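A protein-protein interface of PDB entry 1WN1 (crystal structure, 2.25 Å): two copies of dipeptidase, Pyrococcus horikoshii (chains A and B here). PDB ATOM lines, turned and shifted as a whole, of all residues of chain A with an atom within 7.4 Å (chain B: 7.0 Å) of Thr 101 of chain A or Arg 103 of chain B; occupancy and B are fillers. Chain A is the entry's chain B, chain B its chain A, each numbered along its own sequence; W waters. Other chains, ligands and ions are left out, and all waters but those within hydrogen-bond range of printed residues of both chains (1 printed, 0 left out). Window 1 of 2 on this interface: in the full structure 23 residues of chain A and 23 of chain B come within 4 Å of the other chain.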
ATOM      1  N   SER A  21     -30.227  17.500  -4.464  1.00  0.00           N
ATOM      2  CA  SER A  21     -30.658  16.690  -3.335  1.00  0.00           C
ATOM      3  C   SER A  21     -31.280  17.637  -2.315  1.00  0.00           C
ATOM      4  O   SER A  21     -31.119  18.862  -2.407  1.00  0.00           O
ATOM      5  CB  SER A  21     -29.463  15.967  -2.715  1.00  0.00           C
ATOM      6  OG  SER A  21     -28.326  16.819  -2.686  1.00  0.00           O
ATOM      7  N   PRO A  22     -31.999  17.086  -1.329  1.00  0.00           N
ATOM      8  CA  PRO A  22     -32.631  17.933  -0.308  1.00  0.00           C
ATOM      9  C   PRO A  22     -31.660  18.819   0.454  1.00  0.00           C
ATOM     10  O   PRO A  22     -30.495  18.466   0.643  1.00  0.00           O
ATOM     11  CB  PRO A  22     -33.353  16.925   0.604  1.00  0.00           C
ATOM     12  CG  PRO A  22     -32.669  15.599   0.306  1.00  0.00           C
ATOM     13  CD  PRO A  22     -32.398  15.677  -1.168  1.00  0.00           C
ATOM     14  N   GLY A  23     -32.163  19.977   0.876  1.00  0.00           N
ATOM     15  CA  GLY A  23     -31.364  20.936   1.618  1.00  0.00           C
ATOM     16  C   GLY A  23     -31.877  22.351   1.386  1.00  0.00           C
ATOM     17  O   GLY A  23     -33.014  22.534   0.941  1.00  0.00           O
ATOM     18  N   THR A  24     -31.046  23.351   1.652  1.00  0.00           N
ATOM     19  CA  THR A  24     -31.466  24.732   1.480  1.00  0.00           C
ATOM     20  C   THR A  24     -31.822  25.129   0.041  1.00  0.00           C
ATOM     21  O   THR A  24     -32.853  25.786  -0.178  1.00  0.00           O
ATOM     22  CB  THR A  24     -30.410  25.713   2.046  1.00  0.00           C
ATOM     23  OG1 THR A  24     -29.113  25.414   1.521  1.00  0.00           O
ATOM     24  CG2 THR A  24     -30.350  25.597   3.562  1.00  0.00           C
ATOM     25  N   ASN A  25     -30.995  24.745  -0.936  1.00  0.00           N
ATOM     26  CA  ASN A  25     -31.284  25.090  -2.324  1.00  0.00           C
ATOM     27  C   ASN A  25     -32.581  24.481  -2.814  1.00  0.00           C
ATOM     28  O   ASN A  25     -33.342  25.132  -3.533  1.00  0.00           O
ATOM     29  CB  ASN A  25     -30.151  24.657  -3.253  1.00  0.00           C
ATOM     30  CG  ASN A  25     -28.954  25.575  -3.165  1.00  0.00           C
ATOM     31  OD1 ASN A  25     -29.092  26.803  -3.165  1.00  0.00           O
ATOM     32  ND2 ASN A  25     -27.769  24.987  -3.093  1.00  0.00           N
ATOM     33  N   ILE A  98     -24.646  20.182  -9.788  1.00  0.00           N
ATOM     34  CA  ILE A  98     -24.865  19.246  -8.696  1.00  0.00           C
ATOM     35  C   ILE A  98     -24.925  19.932  -7.325  1.00  0.00           C
ATOM     36  O   ILE A  98     -24.000  20.635  -6.924  1.00  0.00           O
ATOM     37  CB  ILE A  98     -23.717  18.199  -8.665  1.00  0.00           C
ATOM     38  CG1 ILE A  98     -23.721  17.373  -9.961  1.00  0.00           C
ATOM     39  CG2 ILE A  98     -23.826  17.327  -7.424  1.00  0.00           C
ATOM     40  CD1 ILE A  98     -24.824  16.334 -10.005  1.00  0.00           C
ATOM     41  N   GLU A  99     -26.012  19.724  -6.598  1.00  0.00           N
ATOM     42  CA  GLU A  99     -26.130  20.311  -5.267  1.00  0.00           C
ATOM     43  C   GLU A  99     -24.822  20.062  -4.478  1.00  0.00           C
ATOM     44  O   GLU A  99     -24.355  18.931  -4.365  1.00  0.00           O
ATOM     45  CB  GLU A  99     -27.335  19.691  -4.550  1.00  0.00           C
ATOM     46  CG  GLU A  99     -27.337  19.811  -3.032  1.00  0.00           C
ATOM     47  CD  GLU A  99     -27.086  21.226  -2.548  1.00  0.00           C
ATOM     48  OE1 GLU A  99     -27.533  22.174  -3.224  1.00  0.00           O
ATOM     49  OE2 GLU A  99     -26.454  21.377  -1.482  1.00  0.00           O
ATOM     50  N   ASP A 100     -24.250  21.136  -3.944  1.00  0.00           N
ATOM     51  CA  ASP A 100     -22.999  21.108  -3.189  1.00  0.00           C
ATOM     52  C   ASP A 100     -22.913  20.128  -2.024  1.00  0.00           C
ATOM     53  O   ASP A 100     -21.858  19.496  -1.805  1.00  0.00           O
ATOM     54  CB  ASP A 100     -22.676  22.515  -2.654  1.00  0.00           C
ATOM     55  CG  ASP A 100     -22.488  23.536  -3.762  1.00  0.00           C
ATOM     56  OD1 ASP A 100     -23.412  23.741  -4.574  1.00  0.00           O
ATOM     57  OD2 ASP A 100     -21.408  24.138  -3.839  1.00  0.00           O
ATOM     58  N   THR A 101     -24.004  20.006  -1.275  1.00  0.00           N
ATOM     59  CA  THR A 101     -24.050  19.133  -0.101  1.00  0.00           C
ATOM     60  C   THR A 101     -24.504  17.691  -0.340  1.00  0.00           C
ATOM     61  O   THR A 101     -24.621  16.915   0.606  1.00  0.00           O
ATOM     62  CB  THR A 101     -24.983  19.732   0.964  1.00  0.00           C
ATOM     63  OG1 THR A 101     -26.301  19.862   0.410  1.00  0.00           O
ATOM     64  CG2 THR A 101     -24.502  21.105   1.386  1.00  0.00           C
ATOM     65  N   MET A 102     -24.781  17.328  -1.584  1.00  0.00           N
ATOM     66  CA  MET A 102     -25.219  15.959  -1.863  1.00  0.00           C
ATOM     67  C   MET A 102     -24.150  14.959  -1.410  1.00  0.00           C
ATOM     68  O   MET A 102     -22.965  15.250  -1.458  1.00  0.00           O
ATOM     69  CB  MET A 102     -25.463  15.776  -3.355  1.00  0.00           C
ATOM     70  CG  MET A 102     -25.906  14.386  -3.737  1.00  0.00           C
ATOM     71  SD  MET A 102     -25.974  14.173  -5.518  1.00  0.00           S
ATOM     72  CE  MET A 102     -27.091  15.583  -5.992  1.00  0.00           C
ATOM     73  N   ARG A 103     -24.579  13.787  -0.967  1.00  0.00           N
ATOM     74  CA  ARG A 103     -23.647  12.759  -0.541  1.00  0.00           C
ATOM     75  C   ARG A 103     -22.815  12.266  -1.727  1.00  0.00           C
ATOM     76  O   ARG A 103     -23.297  12.186  -2.862  1.00  0.00           O
ATOM     77  CB  ARG A 103     -24.410  11.597   0.074  1.00  0.00           C
ATOM     78  CG  ARG A 103     -25.039  11.907   1.420  1.00  0.00           C
ATOM     79  CD  ARG A 103     -26.010  10.810   1.777  1.00  0.00           C
ATOM     80  NE  ARG A 103     -25.371   9.506   1.818  1.00  0.00           N
ATOM     81  CZ  ARG A 103     -24.979   8.889   2.932  1.00  0.00           C
ATOM     82  NH1 ARG A 103     -25.156   9.456   4.114  1.00  0.00           N
ATOM     83  NH2 ARG A 103     -24.415   7.688   2.860  1.00  0.00           N
ATOM     84  N   ALA A 104     -21.561  11.936  -1.442  1.00  0.00           N
ATOM     85  CA  ALA A 104     -20.628  11.456  -2.441  1.00  0.00           C
ATOM     86  C   ALA A 104     -21.094  10.131  -2.999  1.00  0.00           C
ATOM     87  O   ALA A 104     -20.964   9.894  -4.199  1.00  0.00           O
ATOM     88  CB  ALA A 104     -19.242  11.314  -1.833  1.00  0.00           C
ATOM     89  N   TRP A 106     -24.081   9.202  -3.465  1.00  0.00           N
ATOM     90  CA  TRP A 106     -25.164   9.430  -4.439  1.00  0.00           C
ATOM     91  C   TRP A 106     -24.585   9.870  -5.775  1.00  0.00           C
ATOM     92  O   TRP A 106     -25.023   9.412  -6.842  1.00  0.00           O
ATOM     93  CB  TRP A 106     -26.143  10.509  -3.973  1.00  0.00           C
ATOM     94  CG  TRP A 106     -27.012  10.147  -2.809  1.00  0.00           C
ATOM     95  CD1 TRP A 106     -26.888   9.063  -1.986  1.00  0.00           C
ATOM     96  CD2 TRP A 106     -28.136  10.894  -2.326  1.00  0.00           C
ATOM     97  NE1 TRP A 106     -27.864   9.092  -1.018  1.00  0.00           N
ATOM     98  CE2 TRP A 106     -28.645  10.206  -1.202  1.00  0.00           C
ATOM     99  CE3 TRP A 106     -28.761  12.089  -2.731  1.00  0.00           C
ATOM    100  CZ2 TRP A 106     -29.756  10.663  -0.484  1.00  0.00           C
ATOM    101  CZ3 TRP A 106     -29.864  12.543  -2.014  1.00  0.00           C
ATOM    102  CH2 TRP A 106     -30.346  11.833  -0.902  1.00  0.00           C
ATOM    103  N   LEU A 107     -23.598  10.765  -5.717  1.00  0.00           N
ATOM    104  CA  LEU A 107     -22.950  11.280  -6.925  1.00  0.00           C
ATOM    105  C   LEU A 107     -22.252  10.155  -7.668  1.00  0.00           C
ATOM    106  O   LEU A 107     -22.275  10.098  -8.894  1.00  0.00           O
ATOM    107  CB  LEU A 107     -21.896  12.320  -6.568  1.00  0.00           C
ATOM    108  CG  LEU A 107     -21.772  13.564  -7.436  1.00  0.00           C
ATOM    109  CD1 LEU A 107     -20.336  14.052  -7.348  1.00  0.00           C
ATOM    110  CD2 LEU A 107     -22.189  13.294  -8.876  1.00  0.00           C
ATOM    111  N   LEU A 121     -23.722  23.294  -7.668  1.00  0.00           N
ATOM    112  CA  LEU A 121     -24.922  24.105  -7.870  1.00  0.00           C
ATOM    113  C   LEU A 121     -24.724  25.554  -7.401  1.00  0.00           C
ATOM    114  O   LEU A 121     -25.179  26.483  -8.064  1.00  0.00           O
ATOM    115  CB  LEU A 121     -26.111  23.459  -7.151  1.00  0.00           C
ATOM    116  CG  LEU A 121     -27.466  24.185  -7.136  1.00  0.00           C
ATOM    117  CD1 LEU A 121     -27.906  24.503  -8.556  1.00  0.00           C
ATOM    118  CD2 LEU A 121     -28.500  23.295  -6.444  1.00  0.00           C
ATOM    119  N   SER A 122     -24.023  25.738  -6.281  1.00  0.00           N
ATOM    120  CA  SER A 122     -23.769  27.066  -5.717  1.00  0.00           C
ATOM    121  C   SER A 122     -23.132  28.069  -6.693  1.00  0.00           C
ATOM    122  O   SER A 122     -23.388  29.271  -6.617  1.00  0.00           O
ATOM    123  CB  SER A 122     -22.895  26.948  -4.461  1.00  0.00           C
ATOM    124  OG  SER A 122     -21.613  26.410  -4.753  1.00  0.00           O
ATOM    125  N   ASP A 295     -28.830  29.752   4.956  1.00  0.00           N
ATOM    126  CA  ASP A 295     -27.683  29.157   5.631  1.00  0.00           C
ATOM    127  C   ASP A 295     -26.983  30.219   6.477  1.00  0.00           C
ATOM    128  O   ASP A 295     -27.189  31.438   6.290  1.00  0.00           O
ATOM    129  CB  ASP A 295     -26.668  28.598   4.632  1.00  0.00           C
ATOM    130  CG  ASP A 295     -27.090  27.272   4.055  1.00  0.00           C
ATOM    131  OD1 ASP A 295     -27.337  27.213   2.834  1.00  0.00           O
ATOM    132  OD2 ASP A 295     -27.177  26.294   4.828  1.00  0.00           O
ATOM    133  N   SER B  21     -13.128  11.923   4.174  1.00  0.00           N
ATOM    134  CA  SER B  21     -13.496  13.198   4.769  1.00  0.00           C
ATOM    135  C   SER B  21     -13.876  12.918   6.223  1.00  0.00           C
ATOM    136  O   SER B  21     -14.103  11.772   6.582  1.00  0.00           O
ATOM    137  CB  SER B  21     -14.655  13.827   3.992  1.00  0.00           C
ATOM    138  OG  SER B  21     -15.573  12.835   3.564  1.00  0.00           O
ATOM    139  N   GLY B  38     -17.608  22.015   8.163  1.00  0.00           N
ATOM    140  CA  GLY B  38     -18.357  22.753   7.168  1.00  0.00           C
ATOM    141  C   GLY B  38     -17.840  22.552   5.762  1.00  0.00           C
ATOM    142  O   GLY B  38     -17.720  21.422   5.306  1.00  0.00           O
ATOM    143  N   GLU B  39     -17.512  23.647   5.082  1.00  0.00           N
ATOM    144  CA  GLU B  39     -17.045  23.571   3.700  1.00  0.00           C
ATOM    145  C   GLU B  39     -15.534  23.494   3.537  1.00  0.00           C
ATOM    146  O   GLU B  39     -15.046  23.403   2.409  1.00  0.00           O
ATOM    147  CB  GLU B  39     -17.538  24.781   2.902  1.00  0.00           C
ATOM    148  CG  GLU B  39     -18.825  25.393   3.398  1.00  0.00           C
ATOM    149  CD  GLU B  39     -19.219  26.620   2.594  1.00  0.00           C
ATOM    150  OE1 GLU B  39     -20.057  27.403   3.089  1.00  0.00           O
ATOM    151  OE2 GLU B  39     -18.699  26.807   1.467  1.00  0.00           O
ATOM    152  N   ARG B  40     -14.792  23.540   4.640  1.00  0.00           N
ATOM    153  CA  ARG B  40     -13.335  23.503   4.542  1.00  0.00           C
ATOM    154  C   ARG B  40     -12.799  22.100   4.272  1.00  0.00           C
ATOM    155  O   ARG B  40     -12.936  21.192   5.097  1.00  0.00           O
ATOM    156  CB  ARG B  40     -12.691  24.087   5.806  1.00  0.00           C
ATOM    157  CG  ARG B  40     -12.855  25.605   5.931  1.00  0.00           C
ATOM    158  CD  ARG B  40     -11.909  26.217   6.976  1.00  0.00           C
ATOM    159  NE  ARG B  40     -12.098  27.663   7.116  1.00  0.00           N
ATOM    160  CZ  ARG B  40     -12.979  28.235   7.938  1.00  0.00           C
ATOM    161  NH1 ARG B  40     -13.757  27.486   8.712  1.00  0.00           N
ATOM    162  NH2 ARG B  40     -13.096  29.558   7.974  1.00  0.00           N
ATOM    163  N   TYR B  79      -7.370  22.411  -2.808  1.00  0.00           N
ATOM    164  CA  TYR B  79      -7.407  21.370  -3.814  1.00  0.00           C
ATOM    165  C   TYR B  79      -6.034  21.297  -4.448  1.00  0.00           C
ATOM    166  O   TYR B  79      -5.554  20.217  -4.775  1.00  0.00           O
ATOM    167  CB  TYR B  79      -8.485  21.664  -4.849  1.00  0.00           C
ATOM    168  CG  TYR B  79      -9.859  21.476  -4.270  1.00  0.00           C
ATOM    169  CD1 TYR B  79     -10.416  20.202  -4.149  1.00  0.00           C
ATOM    170  CD2 TYR B  79     -10.566  22.555  -3.735  1.00  0.00           C
ATOM    171  CE1 TYR B  79     -11.640  20.009  -3.501  1.00  0.00           C
ATOM    172  CE2 TYR B  79     -11.785  22.368  -3.086  1.00  0.00           C
ATOM    173  CZ  TYR B  79     -12.311  21.093  -2.973  1.00  0.00           C
ATOM    174  OH  TYR B  79     -13.495  20.907  -2.319  1.00  0.00           O
ATOM    175  N   ILE B  98     -13.981   6.505  -1.620  1.00  0.00           N
ATOM    176  CA  ILE B  98     -14.416   7.846  -1.225  1.00  0.00           C
ATOM    177  C   ILE B  98     -15.364   7.775  -0.042  1.00  0.00           C
ATOM    178  O   ILE B  98     -16.330   7.009  -0.069  1.00  0.00           O
ATOM    179  CB  ILE B  98     -15.172   8.521  -2.387  1.00  0.00           C
ATOM    180  CG1 ILE B  98     -14.258   8.607  -3.608  1.00  0.00           C
ATOM    181  CG2 ILE B  98     -15.689   9.902  -1.966  1.00  0.00           C
ATOM    182  CD1 ILE B  98     -13.085   9.554  -3.443  1.00  0.00           C
ATOM    183  N   GLU B  99     -15.108   8.580   0.986  1.00  0.00           N
ATOM    184  CA  GLU B  99     -15.977   8.580   2.152  1.00  0.00           C
ATOM    185  C   GLU B  99     -17.410   8.803   1.684  1.00  0.00           C
ATOM    186  O   GLU B  99     -17.713   9.812   1.045  1.00  0.00           O
ATOM    187  CB  GLU B  99     -15.566   9.675   3.137  1.00  0.00           C
ATOM    188  CG  GLU B  99     -16.594   9.983   4.234  1.00  0.00           C
ATOM    189  CD  GLU B  99     -17.142   8.737   4.930  1.00  0.00           C
ATOM    190  OE1 GLU B  99     -16.417   7.732   5.021  1.00  0.00           O
ATOM    191  OE2 GLU B  99     -18.298   8.769   5.409  1.00  0.00           O
ATOM    192  N   ASP B 100     -18.278   7.847   1.996  1.00  0.00           N
ATOM    193  CA  ASP B 100     -19.668   7.910   1.599  1.00  0.00           C
ATOM    194  C   ASP B 100     -20.319   9.261   1.858  1.00  0.00           C
ATOM    195  O   ASP B 100     -20.996   9.797   0.980  1.00  0.00           O
ATOM    196  CB  ASP B 100     -20.451   6.822   2.333  1.00  0.00           C
ATOM    197  CG  ASP B 100     -20.013   5.429   1.931  1.00  0.00           C
ATOM    198  OD1 ASP B 100     -18.801   5.144   1.999  1.00  0.00           O
ATOM    199  OD2 ASP B 100     -20.881   4.631   1.538  1.00  0.00           O
ATOM    200  N   THR B 101     -20.096   9.811   3.057  1.00  0.00           N
ATOM    201  CA  THR B 101     -20.695  11.086   3.460  1.00  0.00           C
ATOM    202  C   THR B 101     -19.969  12.361   3.036  1.00  0.00           C
ATOM    203  O   THR B 101     -20.339  13.452   3.483  1.00  0.00           O
ATOM    204  CB  THR B 101     -20.840  11.175   4.966  1.00  0.00           C
ATOM    205  OG1 THR B 101     -19.541  11.310   5.548  1.00  0.00           O
ATOM    206  CG2 THR B 101     -21.523   9.921   5.518  1.00  0.00           C
ATOM    207  N   MET B 102     -18.950  12.237   2.190  1.00  0.00           N
ATOM    208  CA  MET B 102     -18.196  13.400   1.738  1.00  0.00           C
ATOM    209  C   MET B 102     -19.064  14.291   0.868  1.00  0.00           C
ATOM    210  O   MET B 102     -19.866  13.804   0.077  1.00  0.00           O
ATOM    211  CB  MET B 102     -16.962  12.965   0.930  1.00  0.00           C
ATOM    212  CG  MET B 102     -16.130  14.126   0.379  1.00  0.00           C
ATOM    213  SD  MET B 102     -14.741  13.599  -0.672  1.00  0.00           S
ATOM    214  CE  MET B 102     -13.801  12.606   0.474  1.00  0.00           C
ATOM    215  N   ARG B 103     -18.890  15.600   1.003  1.00  0.00           N
ATOM    216  CA  ARG B 103     -19.654  16.539   0.194  1.00  0.00           C
ATOM    217  C   ARG B 103     -19.363  16.368  -1.298  1.00  0.00           C
ATOM    218  O   ARG B 103     -18.215  16.185  -1.716  1.00  0.00           O
ATOM    219  CB  ARG B 103     -19.335  17.982   0.593  1.00  0.00           C
ATOM    220  CG  ARG B 103     -19.832  18.428   1.960  1.00  0.00           C
ATOM    221  CD  ARG B 103     -19.150  19.755   2.330  1.00  0.00           C
ATOM    222  NE  ARG B 103     -19.468  20.815   1.375  1.00  0.00           N
ATOM    223  CZ  ARG B 103     -20.460  21.688   1.536  1.00  0.00           C
ATOM    224  NH1 ARG B 103     -21.215  21.629   2.625  1.00  0.00           N
ATOM    225  NH2 ARG B 103     -20.723  22.597   0.601  1.00  0.00           N
ATOM    226  N   ALA B 104     -20.418  16.459  -2.093  1.00  0.00           N
ATOM    227  CA  ALA B 104     -20.327  16.337  -3.538  1.00  0.00           C
ATOM    228  C   ALA B 104     -19.402  17.396  -4.158  1.00  0.00           C
ATOM    229  O   ALA B 104     -18.672  17.109  -5.115  1.00  0.00           O
ATOM    230  CB  ALA B 104     -21.719  16.440  -4.150  1.00  0.00           C
ATOM    231  N   ASP B 105     -19.434  18.619  -3.633  1.00  0.00           N
ATOM    232  CA  ASP B 105     -18.572  19.644  -4.202  1.00  0.00           C
ATOM    233  C   ASP B 105     -17.085  19.289  -4.003  1.00  0.00           C
ATOM    234  O   ASP B 105     -16.272  19.529  -4.894  1.00  0.00           O
ATOM    235  CB  ASP B 105     -18.943  21.049  -3.668  1.00  0.00           C
ATOM    236  CG  ASP B 105     -18.747  21.213  -2.166  1.00  0.00           C
ATOM    237  OD1 ASP B 105     -18.728  20.224  -1.406  1.00  0.00           O
ATOM    238  OD2 ASP B 105     -18.640  22.375  -1.728  1.00  0.00           O
ATOM    239  N   TRP B 106     -16.738  18.697  -2.860  1.00  0.00           N
ATOM    240  CA  TRP B 106     -15.356  18.273  -2.615  1.00  0.00           C
ATOM    241  C   TRP B 106     -14.988  17.183  -3.619  1.00  0.00           C
ATOM    242  O   TRP B 106     -13.915  17.223  -4.226  1.00  0.00           O
ATOM    243  CB  TRP B 106     -15.181  17.676  -1.223  1.00  0.00           C
ATOM    244  CG  TRP B 106     -15.271  18.644  -0.104  1.00  0.00           C
ATOM    245  CD1 TRP B 106     -15.772  19.917  -0.148  1.00  0.00           C
ATOM    246  CD2 TRP B 106     -14.962  18.381   1.268  1.00  0.00           C
ATOM    247  NE1 TRP B 106     -15.792  20.459   1.119  1.00  0.00           N
ATOM    248  CE2 TRP B 106     -15.298  19.542   1.999  1.00  0.00           C
ATOM    249  CE3 TRP B 106     -14.421  17.285   1.942  1.00  0.00           C
ATOM    250  CZ2 TRP B 106     -15.135  19.620   3.389  1.00  0.00           C
ATOM    251  CZ3 TRP B 106     -14.254  17.361   3.316  1.00  0.00           C
ATOM    252  CH2 TRP B 106     -14.604  18.527   4.028  1.00  0.00           C
ATOM    253  N   LEU B 107     -15.880  16.209  -3.792  1.00  0.00           N
ATOM    254  CA  LEU B 107     -15.615  15.110  -4.714  1.00  0.00           C
ATOM    255  C   LEU B 107     -15.421  15.645  -6.120  1.00  0.00           C
ATOM    256  O   LEU B 107     -14.548  15.188  -6.856  1.00  0.00           O
ATOM    257  CB  LEU B 107     -16.772  14.107  -4.725  1.00  0.00           C
ATOM    258  CG  LEU B 107     -16.462  12.635  -5.052  1.00  0.00           C
ATOM    259  CD1 LEU B 107     -17.665  12.029  -5.768  1.00  0.00           C
ATOM    260  CD2 LEU B 107     -15.208  12.493  -5.894  1.00  0.00           C
ATOM    261  N   ILE B 108     -16.255  16.608  -6.489  1.00  0.00           N
ATOM    262  CA  ILE B 108     -16.190  17.209  -7.808  1.00  0.00           C
ATOM    263  C   ILE B 108     -14.860  17.910  -8.004  1.00  0.00           C
ATOM    264  O   ILE B 108     -14.295  17.879  -9.095  1.00  0.00           O
ATOM    265  CB  ILE B 108     -17.322  18.217  -8.010  1.00  0.00           C
ATOM    266  CG1 ILE B 108     -18.641  17.476  -8.204  1.00  0.00           C
ATOM    267  CG2 ILE B 108     -16.999  19.126  -9.175  1.00  0.00           C
ATOM    268  CD1 ILE B 108     -19.857  18.370  -8.180  1.00  0.00           C
ATOM    269  N   GLY B 109     -14.363  18.544  -6.947  1.00  0.00           N
ATOM    270  CA  GLY B 109     -13.084  19.229  -7.032  1.00  0.00           C
ATOM    271  C   GLY B 109     -11.962  18.213  -7.131  1.00  0.00           C
ATOM    272  O   GLY B 109     -10.996  18.377  -7.883  1.00  0.00           O
ATOM    273  N   ILE B 110     -12.102  17.141  -6.365  1.00  0.00           N
ATOM    274  CA  ILE B 110     -11.115  16.084  -6.376  1.00  0.00           C
ATOM    275  C   ILE B 110     -11.048  15.503  -7.782  1.00  0.00           C
ATOM    276  O   ILE B 110      -9.981  15.137  -8.251  1.00  0.00           O
ATOM    277  CB  ILE B 110     -11.490  14.997  -5.369  1.00  0.00           C
ATOM    278  CG1 ILE B 110     -11.177  15.487  -3.954  1.00  0.00           C
ATOM    279  CG2 ILE B 110     -10.764  13.715  -5.694  1.00  0.00           C
ATOM    280  CD1 ILE B 110     -11.811  14.647  -2.854  1.00  0.00           C
HETATM  281  O   HOH W   1     -19.091  24.802  -3.515  1.00  0.00           O
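The backbone carbonyl oxygen (O) of Asp 100 of chain B sits at hydrogen-bond distance from the backbone NH (N) of Ala 104 of chain A (3.3 Å).
N of Ala 104 of chain A is in hydrogen-bond range of O of Met 102 of chain B, at 2.9 Å.
The backbone NH (N) of Ala 104 of chain B is in hydrogen-bond range of the backbone carbonyl oxygen (O) of Asp 100 of chain A (3.4 Å).
The backbone carbonyl oxygen (O) of Met 102 of chain A sits at hydrogen-bond distance from the backbone NH (N) of Ala 104 of chain B.
O of Asp 100 of chain A lies within hydrogen-bond range of N of Asp 105 of chain B (3.2 Å).
OE2 of Glu 99 of chain B sits at hydrogen-bond distance from OG1 of Thr 101 of chain B (2.8 Å).
The guanidinium group (NE) of Arg 103 of chain B is in salt-bridge range of the side-chain carboxylate (OD1) of Asp 105 of chain B (2.9 Å).
The side-chain carboxylate (OE1) of Glu 99 of chain A lies within hydrogen-bond range of the side-chain amide nitrogen (ND2) of Asn 25 of chain A, 2.8 Å away.
The backbone carbonyl oxygen (O) of Ile 98 of chain A sits at hydrogen-bond distance from the backbone NH (N) of Leu 121 of chain A (2.8 Å).
The side-chain carboxylate (OE2) of Glu 99 of chain A is in hydrogen-bond range of the side-chain hydroxyl (OG1) of Thr 101 of chain A (2.4 Å).
The side-chain carboxylate of Asp 100 of chain A is in hydrogen-bond range of the side-chain hydroxyl of Ser 122 of chain A (2.5 Å).
Among the printed residues, pairs that only touch across the chains: Ile 98 of chain A with Ala 104 of chain B (3.99 Å), Ile 98 of chain A with Ile 108 of chain B (3.9 Å), Glu 99 of chain A with Ala 104 of chain B (3.6 Å), Asp 100 of chain A with Arg 103 of chain B (3.8 Å), Thr 101 of chain A with Arg 103 of chain B (3.6 Å), Met 102 of chain A with Met 102 of chain B (3.7 Å), Met 102 of chain A with Arg 103 of chain B (3.8 Å), Arg 103 of chain A with Asp 100 of chain B (3.96 Å), Arg 103 of chain A with Thr 101 of chain B (3.9 Å), Arg 103 of chain A with Met 102 of chain B (3.8 Å), Ala 104 of chain A with Ile 98 of chain B (3.8 Å), Ala 104 of chain A with Glu 99 of chain B (3.6 Å), Leu 107 of chain A with Leu 107 of chain B (3.7 Å) and Leu 107 of chain A with Ile 108 of chain B (3.9 Å).
Printed residues of chain B within 4 Å of Glu 99 of chain A: Ala 104.
Of the printed residues of chain B, Met 102 of chain A touches Met 102 (3.7 Å), Arg 103 (3.8 Å) and Ala 104 (2.9 Å).
Of the printed residues of chain A, Asp 100 of chain B touches Arg 103 and Ala 104.
Of the printed residues of chain A, Arg 103 of chain B touches Asp 100 (3.8 Å), Thr 101 (3.6 Å) and Met 102 (3.8 Å).
Of the 17 printed residues of chain A, 8 touch a printed residue of chain B.
Hydrophobic or aromatic side chains of chain A within 4 Å of the printed part of chain B: Ile 98, Met 102, Ala 104 and Leu 107.
Along chain A the printed residues that touch a printed residue of chain B span positions 98 to 107.
Among the printed residues, no Asp or Glu carboxylate lies within 4 Å of a Lys or Arg side-chain nitrogen of the other chain.
Asp 100 of chain A touches Arg 103 of chain B, and with the chains exchanged Arg 103 of chain A touches Asp 100 of chain B.
Asp 100 of chain A touches Ala 104 of chain B, and with the chains exchanged Ala 104 of chain A touches Asp 100 of chain B.
Met 102 of chain A touches Arg 103 of chain B, and with the chains exchanged Arg 103 of chain A touches Met 102 of chain B.
Met 102 of chain A touches Ala 104 of chain B, and with the chains exchanged Ala 104 of chain A touches Met 102 of chain B.
Positions printed for both chains: 21, 98, 99, 100, 101, 102, 103, 104, 106 and 107.
Of the 19 pairs that touch across the chains among the printed residues, 16 have their exchanged pair printed and touching as well.
Water W1 lies within hydrogen-bond range of OD2 of Asp 100 of chain A, OD2 of Asp 105 of chain B and OG of Ser 122 of chain A.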
